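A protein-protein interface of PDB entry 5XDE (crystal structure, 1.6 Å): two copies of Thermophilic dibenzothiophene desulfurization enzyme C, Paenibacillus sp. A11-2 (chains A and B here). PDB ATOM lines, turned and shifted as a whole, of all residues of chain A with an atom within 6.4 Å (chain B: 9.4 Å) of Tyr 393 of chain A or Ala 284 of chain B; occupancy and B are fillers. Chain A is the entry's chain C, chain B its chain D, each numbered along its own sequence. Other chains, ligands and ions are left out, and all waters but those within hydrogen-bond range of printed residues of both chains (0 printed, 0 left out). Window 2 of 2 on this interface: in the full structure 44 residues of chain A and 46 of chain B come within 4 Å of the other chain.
The side-chain hydroxyl (OH) of Tyr 393 of chain A sits at hydrogen-bond distance from the side-chain carboxylate (OD2) of Asp 292 of chain B (2.6 Å).
The backbone carbonyl oxygen (O) of Phe 281 of chain B sits at hydrogen-bond distance from the backbone NH (N) of Val 286 of chain B.
OD1 of Asp 292 of chain B lies within hydrogen-bond range of N of Tyr 294 of chain B (2.8 Å).
OD1 of Asp 292 of chain B lies within hydrogen-bond range of N of Val 295 of chain B (3.0 Å).
Pro 390 of chain A touches Phe 281 of chain B.
Tyr 294 of chain B touches Ala 392 of chain A.
CD2 of Tyr 393 of chain A touches CD2 of Phe 281 of chain B, at 3.5 Å.
Tyr 393 of chain A touches Ala 284 of chain B (CE1 to CB, 3.3 Å).
CG2 of Val 286 of chain B touches OH of Tyr 393 of chain A (3.3 Å).
Tyr 393 of chain A touches Tyr 294 of chain B.
OH of Tyr 294 of chain B touches CG of Arg 396 of chain A (3.8 Å).
Of the printed residues of chain B, Pro 390 of chain A touches Phe 281.
Of chain B, only Phe 281 (3.5 Å), Ala 284 (3.3 Å), Val 286 (3.3 Å), Asp 292 (2.6 Å) and Tyr 294 (3.7 Å) come within 4 Å of Tyr 393 of chain A.
Of the printed residues of chain B, Arg 396 of chain A touches Tyr 294.
Pro 280 of chain B touches none of the printed residues of chain A.
Ala 284 of chain B touches one residue of chain A.
Hydrophobic or aromatic side chains of chain B within 4 Å of the printed part of chain A: Phe 281, Ala 284, Val 286 and Tyr 294.
Of the 9 printed residues of chain A, 4 touch a printed residue of chain B.
Among the printed residues, 8 pairs touch across the chains.
Among the printed residues, no Asp or Glu carboxylate lies within 4 Å of a Lys or Arg side-chain nitrogen of the other chain.
No position is printed for both chains.
Of the 8 pairs that touch across the chains among the printed residues, none has its exchanged pair printed and touching as well.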
ATOM      1  N   PRO A 390      17.334   6.504  32.214  1.00  0.00           N
ATOM      2  CA  PRO A 390      17.212   7.885  31.708  1.00  0.00           C
ATOM      3  C   PRO A 390      15.906   8.120  30.954  1.00  0.00           C
ATOM      4  O   PRO A 390      15.585   7.430  29.982  1.00  0.00           O
ATOM      5  CB  PRO A 390      18.429   8.042  30.796  1.00  0.00           C
ATOM      6  CG  PRO A 390      18.834   6.633  30.430  1.00  0.00           C
ATOM      7  CD  PRO A 390      18.450   5.767  31.600  1.00  0.00           C
ATOM      8  N   VAL A 391      15.168   9.144  31.389  1.00  0.00           N
ATOM      9  CA  VAL A 391      13.900   9.433  30.747  1.00  0.00           C
ATOM     10  C   VAL A 391      14.093   9.869  29.302  1.00  0.00           C
ATOM     11  O   VAL A 391      13.178   9.716  28.494  1.00  0.00           O
ATOM     12  CB  VAL A 391      13.122  10.489  31.548  1.00  0.00           C
ATOM     13  CG1 VAL A 391      13.754  11.860  31.402  1.00  0.00           C
ATOM     14  CG2 VAL A 391      11.655  10.499  31.126  1.00  0.00           C
ATOM     15  N   ALA A 392      15.262  10.402  28.949  1.00  0.00           N
ATOM     16  CA  ALA A 392      15.491  10.767  27.553  1.00  0.00           C
ATOM     17  C   ALA A 392      15.351   9.564  26.635  1.00  0.00           C
ATOM     18  O   ALA A 392      14.912   9.702  25.486  1.00  0.00           O
ATOM     19  CB  ALA A 392      16.870  11.394  27.389  1.00  0.00           C
ATOM     20  N   TYR A 393      15.733   8.374  27.108  1.00  0.00           N
ATOM     21  CA  TYR A 393      15.619   7.199  26.259  1.00  0.00           C
ATOM     22  C   TYR A 393      14.252   6.542  26.320  1.00  0.00           C
ATOM     23  O   TYR A 393      13.874   5.865  25.362  1.00  0.00           O
ATOM     24  CB  TYR A 393      16.746   6.204  26.578  1.00  0.00           C
ATOM     25  CG  TYR A 393      18.020   6.760  26.002  1.00  0.00           C
ATOM     26  CD1 TYR A 393      18.305   6.614  24.654  1.00  0.00           C
ATOM     27  CD2 TYR A 393      18.891   7.516  26.783  1.00  0.00           C
ATOM     28  CE1 TYR A 393      19.439   7.181  24.098  1.00  0.00           C
ATOM     29  CE2 TYR A 393      20.036   8.078  26.238  1.00  0.00           C
ATOM     30  CZ  TYR A 393      20.303   7.901  24.893  1.00  0.00           C
ATOM     31  OH  TYR A 393      21.426   8.463  24.329  1.00  0.00           O
ATOM     32  N   LYS A 394      13.471   6.769  27.378  1.00  0.00           N
ATOM     33  CA  LYS A 394      12.051   6.449  27.279  1.00  0.00           C
ATOM     34  C   LYS A 394      11.375   7.327  26.226  1.00  0.00           C
ATOM     35  O   LYS A 394      10.557   6.844  25.434  1.00  0.00           O
ATOM     36  CB  LYS A 394      11.390   6.604  28.644  1.00  0.00           C
ATOM     37  CG  LYS A 394      11.853   5.539  29.659  1.00  0.00           C
ATOM     38  CD  LYS A 394      11.092   4.234  29.450  1.00  0.00           C
ATOM     39  CE  LYS A 394      11.859   3.037  30.025  1.00  0.00           C
ATOM     40  NZ  LYS A 394      12.994   2.653  29.158  1.00  0.00           N
ATOM     41  N   ILE A 395      11.723   8.616  26.190  1.00  0.00           N
ATOM     42  CA  ILE A 395      11.177   9.515  25.169  1.00  0.00           C
ATOM     43  C   ILE A 395      11.562   9.031  23.770  1.00  0.00           C
ATOM     44  O   ILE A 395      10.718   8.959  22.864  1.00  0.00           O
ATOM     45  CB  ILE A 395      11.643  10.960  25.435  1.00  0.00           C
ATOM     46  CG1 ILE A 395      10.897  11.523  26.655  1.00  0.00           C
ATOM     47  CG2 ILE A 395      11.428  11.861  24.215  1.00  0.00           C
ATOM     48  CD1 ILE A 395      11.551  12.757  27.250  1.00  0.00           C
ATOM     49  N   ARG A 396      12.838   8.663  23.582  1.00  0.00           N
ATOM     50  CA  ARG A 396      13.278   8.137  22.288  1.00  0.00           C
ATOM     51  C   ARG A 396      12.506   6.878  21.914  1.00  0.00           C
ATOM     52  O   ARG A 396      12.114   6.705  20.756  1.00  0.00           O
ATOM     53  CB  ARG A 396      14.780   7.843  22.308  1.00  0.00           C
ATOM     54  CG  ARG A 396      15.356   7.591  20.905  1.00  0.00           C
ATOM     55  CD  ARG A 396      16.779   7.055  20.973  1.00  0.00           C
ATOM     56  NE  ARG A 396      17.389   6.991  19.638  1.00  0.00           N
ATOM     57  CZ  ARG A 396      17.173   6.008  18.767  1.00  0.00           C
ATOM     58  NH1 ARG A 396      16.360   5.006  19.081  1.00  0.00           N
ATOM     59  NH2 ARG A 396      17.771   6.027  17.580  1.00  0.00           N
ATOM     60  N   GLU A 397      12.264   5.997  22.889  1.00  0.00           N
ATOM     61  CA  GLU A 397      11.517   4.772  22.625  1.00  0.00           C
ATOM     62  C   GLU A 397      10.093   5.074  22.156  1.00  0.00           C
ATOM     63  O   GLU A 397       9.620   4.481  21.178  1.00  0.00           O
ATOM     64  CB  GLU A 397      11.532   3.881  23.872  1.00  0.00           C
ATOM     65  CG  GLU A 397      12.893   3.216  24.076  1.00  0.00           C
ATOM     66  CD  GLU A 397      13.187   2.884  25.531  1.00  0.00           C
ATOM     67  OE1 GLU A 397      12.262   2.961  26.366  1.00  0.00           O
ATOM     68  OE2 GLU A 397      14.358   2.563  25.828  1.00  0.00           O
ATOM     69  N   VAL A 398       9.414   6.032  22.797  1.00  0.00           N
ATOM     70  CA  VAL A 398       8.069   6.379  22.347  1.00  0.00           C
ATOM     71  C   VAL A 398       8.119   7.021  20.966  1.00  0.00           C
ATOM     72  O   VAL A 398       7.254   6.774  20.119  1.00  0.00           O
ATOM     73  CB  VAL A 398       7.381   7.299  23.372  1.00  0.00           C
ATOM     74  CG1 VAL A 398       6.034   7.772  22.834  1.00  0.00           C
ATOM     75  CG2 VAL A 398       7.204   6.571  24.692  1.00  0.00           C
ATOM     76  N   ARG B 279      28.322   7.296  33.065  1.00  0.00           N
ATOM     77  CA  ARG B 279      28.514   6.108  32.247  1.00  0.00           C
ATOM     78  C   ARG B 279      27.696   6.193  30.966  1.00  0.00           C
ATOM     79  O   ARG B 279      26.584   6.734  30.975  1.00  0.00           O
ATOM     80  CB  ARG B 279      28.119   4.858  33.030  1.00  0.00           C
ATOM     81  CG  ARG B 279      28.994   4.629  34.239  1.00  0.00           C
ATOM     82  CD  ARG B 279      28.624   3.345  34.966  1.00  0.00           C
ATOM     83  NE  ARG B 279      27.276   3.397  35.526  1.00  0.00           N
ATOM     84  CZ  ARG B 279      26.681   2.365  36.121  1.00  0.00           C
ATOM     85  NH1 ARG B 279      27.322   1.200  36.231  1.00  0.00           N
ATOM     86  NH2 ARG B 279      25.453   2.486  36.602  1.00  0.00           N
ATOM     87  N   PRO B 280      28.218   5.677  29.849  1.00  0.00           N
ATOM     88  CA  PRO B 280      27.477   5.767  28.589  1.00  0.00           C
ATOM     89  C   PRO B 280      26.286   4.827  28.600  1.00  0.00           C
ATOM     90  O   PRO B 280      26.351   3.720  29.143  1.00  0.00           O
ATOM     91  CB  PRO B 280      28.514   5.354  27.537  1.00  0.00           C
ATOM     92  CG  PRO B 280      29.419   4.404  28.288  1.00  0.00           C
ATOM     93  CD  PRO B 280      29.503   4.963  29.692  1.00  0.00           C
ATOM     94  N   PHE B 281      25.177   5.281  28.012  1.00  0.00           N
ATOM     95  CA  PHE B 281      23.993   4.431  27.903  1.00  0.00           C
ATOM     96  C   PHE B 281      24.200   3.502  26.709  1.00  0.00           C
ATOM     97  O   PHE B 281      23.681   3.709  25.609  1.00  0.00           O
ATOM     98  CB  PHE B 281      22.722   5.266  27.784  1.00  0.00           C
ATOM     99  CG  PHE B 281      21.471   4.491  28.082  1.00  0.00           C
ATOM    100  CD1 PHE B 281      21.303   3.864  29.307  1.00  0.00           C
ATOM    101  CD2 PHE B 281      20.465   4.379  27.137  1.00  0.00           C
ATOM    102  CE1 PHE B 281      20.148   3.133  29.578  1.00  0.00           C
ATOM    103  CE2 PHE B 281      19.310   3.655  27.403  1.00  0.00           C
ATOM    104  CZ  PHE B 281      19.151   3.034  28.624  1.00  0.00           C
ATOM    105  N   THR B 282      24.990   2.446  26.947  1.00  0.00           N
ATOM    106  CA  THR B 282      25.328   1.509  25.877  1.00  0.00           C
ATOM    107  C   THR B 282      24.094   0.831  25.296  1.00  0.00           C
ATOM    108  O   THR B 282      24.085   0.482  24.107  1.00  0.00           O
ATOM    109  CB  THR B 282      26.320   0.457  26.392  1.00  0.00           C
ATOM    110  OG1 THR B 282      25.812  -0.139  27.592  1.00  0.00           O
ATOM    111  CG2 THR B 282      27.663   1.098  26.679  1.00  0.00           C
ATOM    112  N   LEU B 283      23.051   0.624  26.107  1.00  0.00           N
ATOM    113  CA  LEU B 283      21.789   0.069  25.624  1.00  0.00           C
ATOM    114  C   LEU B 283      21.374   0.735  24.320  1.00  0.00           C
ATOM    115  O   LEU B 283      20.802   0.091  23.439  1.00  0.00           O
ATOM    116  CB  LEU B 283      20.665   0.260  26.651  1.00  0.00           C
ATOM    117  CG  LEU B 283      20.299  -0.736  27.763  1.00  0.00           C
ATOM    118  CD1 LEU B 283      20.190  -2.161  27.225  1.00  0.00           C
ATOM    119  CD2 LEU B 283      21.261  -0.650  28.932  1.00  0.00           C
ATOM    120  N   ALA B 284      21.629   2.035  24.199  1.00  0.00           N
ATOM    121  CA  ALA B 284      21.220   2.799  23.033  1.00  0.00           C
ATOM    122  C   ALA B 284      22.373   3.076  22.081  1.00  0.00           C
ATOM    123  O   ALA B 284      22.236   3.921  21.190  1.00  0.00           O
ATOM    124  CB  ALA B 284      20.576   4.116  23.470  1.00  0.00           C
ATOM    125  N   GLY B 285      23.508   2.405  22.255  1.00  0.00           N
ATOM    126  CA  GLY B 285      24.627   2.552  21.349  1.00  0.00           C
ATOM    127  C   GLY B 285      25.581   3.681  21.664  1.00  0.00           C
ATOM    128  O   GLY B 285      26.513   3.921  20.886  1.00  0.00           O
ATOM    129  N   VAL B 286      25.378   4.384  22.777  1.00  0.00           N
ATOM    130  CA  VAL B 286      26.287   5.451  23.173  1.00  0.00           C
ATOM    131  C   VAL B 286      27.597   4.851  23.664  1.00  0.00           C
ATOM    132  O   VAL B 286      27.606   3.882  24.434  1.00  0.00           O
ATOM    133  CB  VAL B 286      25.640   6.321  24.263  1.00  0.00           C
ATOM    134  CG1 VAL B 286      26.633   7.363  24.758  1.00  0.00           C
ATOM    135  CG2 VAL B 286      24.364   6.987  23.745  1.00  0.00           C
ATOM    136  N   GLU B 287      28.716   5.444  23.249  1.00  0.00           N
ATOM    137  CA  GLU B 287      30.026   4.977  23.684  1.00  0.00           C
ATOM    138  C   GLU B 287      30.668   5.858  24.742  1.00  0.00           C
ATOM    139  O   GLU B 287      31.434   5.350  25.568  1.00  0.00           O
ATOM    140  CB  GLU B 287      30.973   4.858  22.483  1.00  0.00           C
ATOM    141  CG  GLU B 287      30.491   3.868  21.443  1.00  0.00           C
ATOM    142  CD  GLU B 287      31.503   3.628  20.332  1.00  0.00           C
ATOM    143  OE1 GLU B 287      31.443   2.545  19.712  1.00  0.00           O
ATOM    144  OE2 GLU B 287      32.351   4.511  20.076  1.00  0.00           O
ATOM    145  N   LYS B 288      30.380   7.158  24.744  1.00  0.00           N
ATOM    146  CA  LYS B 288      30.881   8.089  25.746  1.00  0.00           C
ATOM    147  C   LYS B 288      29.723   8.950  26.214  1.00  0.00           C
ATOM    148  O   LYS B 288      28.967   9.472  25.385  1.00  0.00           O
ATOM    149  CB  LYS B 288      31.983   9.001  25.185  1.00  0.00           C
ATOM    150  CG  LYS B 288      33.336   8.356  24.962  1.00  0.00           C
ATOM    151  CD  LYS B 288      34.336   9.422  24.499  1.00  0.00           C
ATOM    152  CE  LYS B 288      35.651   8.823  24.013  1.00  0.00           C
ATOM    153  NZ  LYS B 288      36.567   9.879  23.494  1.00  0.00           N
ATOM    154  N   ALA B 289      29.589   9.114  27.531  1.00  0.00           N
ATOM    155  CA  ALA B 289      28.526   9.975  28.039  1.00  0.00           C
ATOM    156  C   ALA B 289      28.675  11.407  27.540  1.00  0.00           C
ATOM    157  O   ALA B 289      27.671  12.102  27.338  1.00  0.00           O
ATOM    158  CB  ALA B 289      28.500   9.946  29.564  1.00  0.00           C
ATOM    159  N   GLU B 291      29.459  12.320  24.685  1.00  0.00           N
ATOM    160  CA  GLU B 291      28.952  12.396  23.320  1.00  0.00           C
ATOM    161  C   GLU B 291      27.467  12.069  23.248  1.00  0.00           C
ATOM    162  O   GLU B 291      26.909  11.963  22.150  1.00  0.00           O
ATOM    163  CB  GLU B 291      29.744  11.461  22.401  1.00  0.00           C
ATOM    164  CG  GLU B 291      31.240  11.814  22.280  1.00  0.00           C
ATOM    165  CD  GLU B 291      31.482  13.251  21.819  1.00  0.00           C
ATOM    166  OE1 GLU B 291      32.412  13.909  22.340  1.00  0.00           O
ATOM    167  OE2 GLU B 291      30.740  13.729  20.928  1.00  0.00           O
ATOM    168  N   ASP B 292      26.811  11.911  24.384  1.00  0.00           N
ATOM    169  CA  ASP B 292      25.410  11.552  24.364  1.00  0.00           C
ATOM    170  C   ASP B 292      24.586  12.740  23.879  1.00  0.00           C
ATOM    171  O   ASP B 292      24.725  13.838  24.423  1.00  0.00           O
ATOM    172  CB  ASP B 292      24.957  11.126  25.756  1.00  0.00           C
ATOM    173  CG  ASP B 292      23.507  10.687  25.787  1.00  0.00           C
ATOM    174  OD1 ASP B 292      22.625  11.564  25.749  1.00  0.00           O
ATOM    175  OD2 ASP B 292      23.246   9.472  25.866  1.00  0.00           O
ATOM    176  N   PRO B 293      23.721  12.567  22.880  1.00  0.00           N
ATOM    177  CA  PRO B 293      23.021  13.747  22.336  1.00  0.00           C
ATOM    178  C   PRO B 293      22.135  14.441  23.349  1.00  0.00           C
ATOM    179  O   PRO B 293      21.978  15.670  23.284  1.00  0.00           O
ATOM    180  CB  PRO B 293      22.209  13.170  21.167  1.00  0.00           C
ATOM    181  CG  PRO B 293      22.067  11.706  21.488  1.00  0.00           C
ATOM    182  CD  PRO B 293      23.364  11.333  22.158  1.00  0.00           C
ATOM    183  N   TYR B 294      21.560  13.700  24.300  1.00  0.00           N
ATOM    184  CA  TYR B 294      20.637  14.326  25.244  1.00  0.00           C
ATOM    185  C   TYR B 294      21.372  14.961  26.416  1.00  0.00           C
ATOM    186  O   TYR B 294      20.922  15.992  26.937  1.00  0.00           O
ATOM    187  CB  TYR B 294      19.596  13.293  25.699  1.00  0.00           C
ATOM    188  CG  TYR B 294      18.904  12.643  24.507  1.00  0.00           C
ATOM    189  CD1 TYR B 294      18.256  13.424  23.562  1.00  0.00           C
ATOM    190  CD2 TYR B 294      18.921  11.265  24.317  1.00  0.00           C
ATOM    191  CE1 TYR B 294      17.637  12.855  22.459  1.00  0.00           C
ATOM    192  CE2 TYR B 294      18.290  10.681  23.199  1.00  0.00           C
ATOM    193  CZ  TYR B 294      17.647  11.496  22.286  1.00  0.00           C
ATOM    194  OH  TYR B 294      17.013  10.986  21.176  1.00  0.00           O
ATOM    195  N   VAL B 295      22.510  14.382  26.821  1.00  0.00           N
ATOM    196  CA  VAL B 295      23.417  15.063  27.743  1.00  0.00           C
ATOM    197  C   VAL B 295      23.874  16.387  27.148  1.00  0.00           C
ATOM    198  O   VAL B 295      23.845  17.432  27.810  1.00  0.00           O
ATOM    199  CB  VAL B 295      24.616  14.154  28.078  1.00  0.00           C
ATOM    200  CG1 VAL B 295      25.666  14.931  28.890  1.00  0.00           C
ATOM    201  CG2 VAL B 295      24.130  12.885  28.812  1.00  0.00           C
ATOM    202  N   LEU B 296      24.302  16.359  25.881  1.00  0.00           N
ATOM    203  CA  LEU B 296      24.813  17.568  25.241  1.00  0.00           C
ATOM    204  C   LEU B 296      23.728  18.632  25.129  1.00  0.00           C
ATOM    205  O   LEU B 296      23.997  19.825  25.304  1.00  0.00           O
ATOM    206  CB  LEU B 296      25.393  17.228  23.862  1.00  0.00           C
ATOM    207  CG  LEU B 296      26.785  16.577  23.872  1.00  0.00           C
ATOM    208  CD1 LEU B 296      27.186  16.058  22.496  1.00  0.00           C
ATOM    209  CD2 LEU B 296      27.824  17.561  24.399  1.00  0.00           C
ATOM    210  N   GLU B 361      19.776  14.870  35.277  1.00  0.00           N
ATOM    211  CA  GLU B 361      19.539  14.034  34.109  1.00  0.00           C
ATOM    212  C   GLU B 361      20.748  13.958  33.185  1.00  0.00           C
ATOM    213  O   GLU B 361      20.841  13.022  32.390  1.00  0.00           O
ATOM    214  CB  GLU B 361      18.303  14.547  33.366  1.00  0.00           C
ATOM    215  CG  GLU B 361      17.036  14.383  34.201  1.00  0.00           C
ATOM    216  CD  GLU B 361      15.909  15.306  33.757  1.00  0.00           C
ATOM    217  OE1 GLU B 361      15.320  16.010  34.625  1.00  0.00           O
ATOM    218  OE2 GLU B 361      15.624  15.312  32.537  1.00  0.00           O
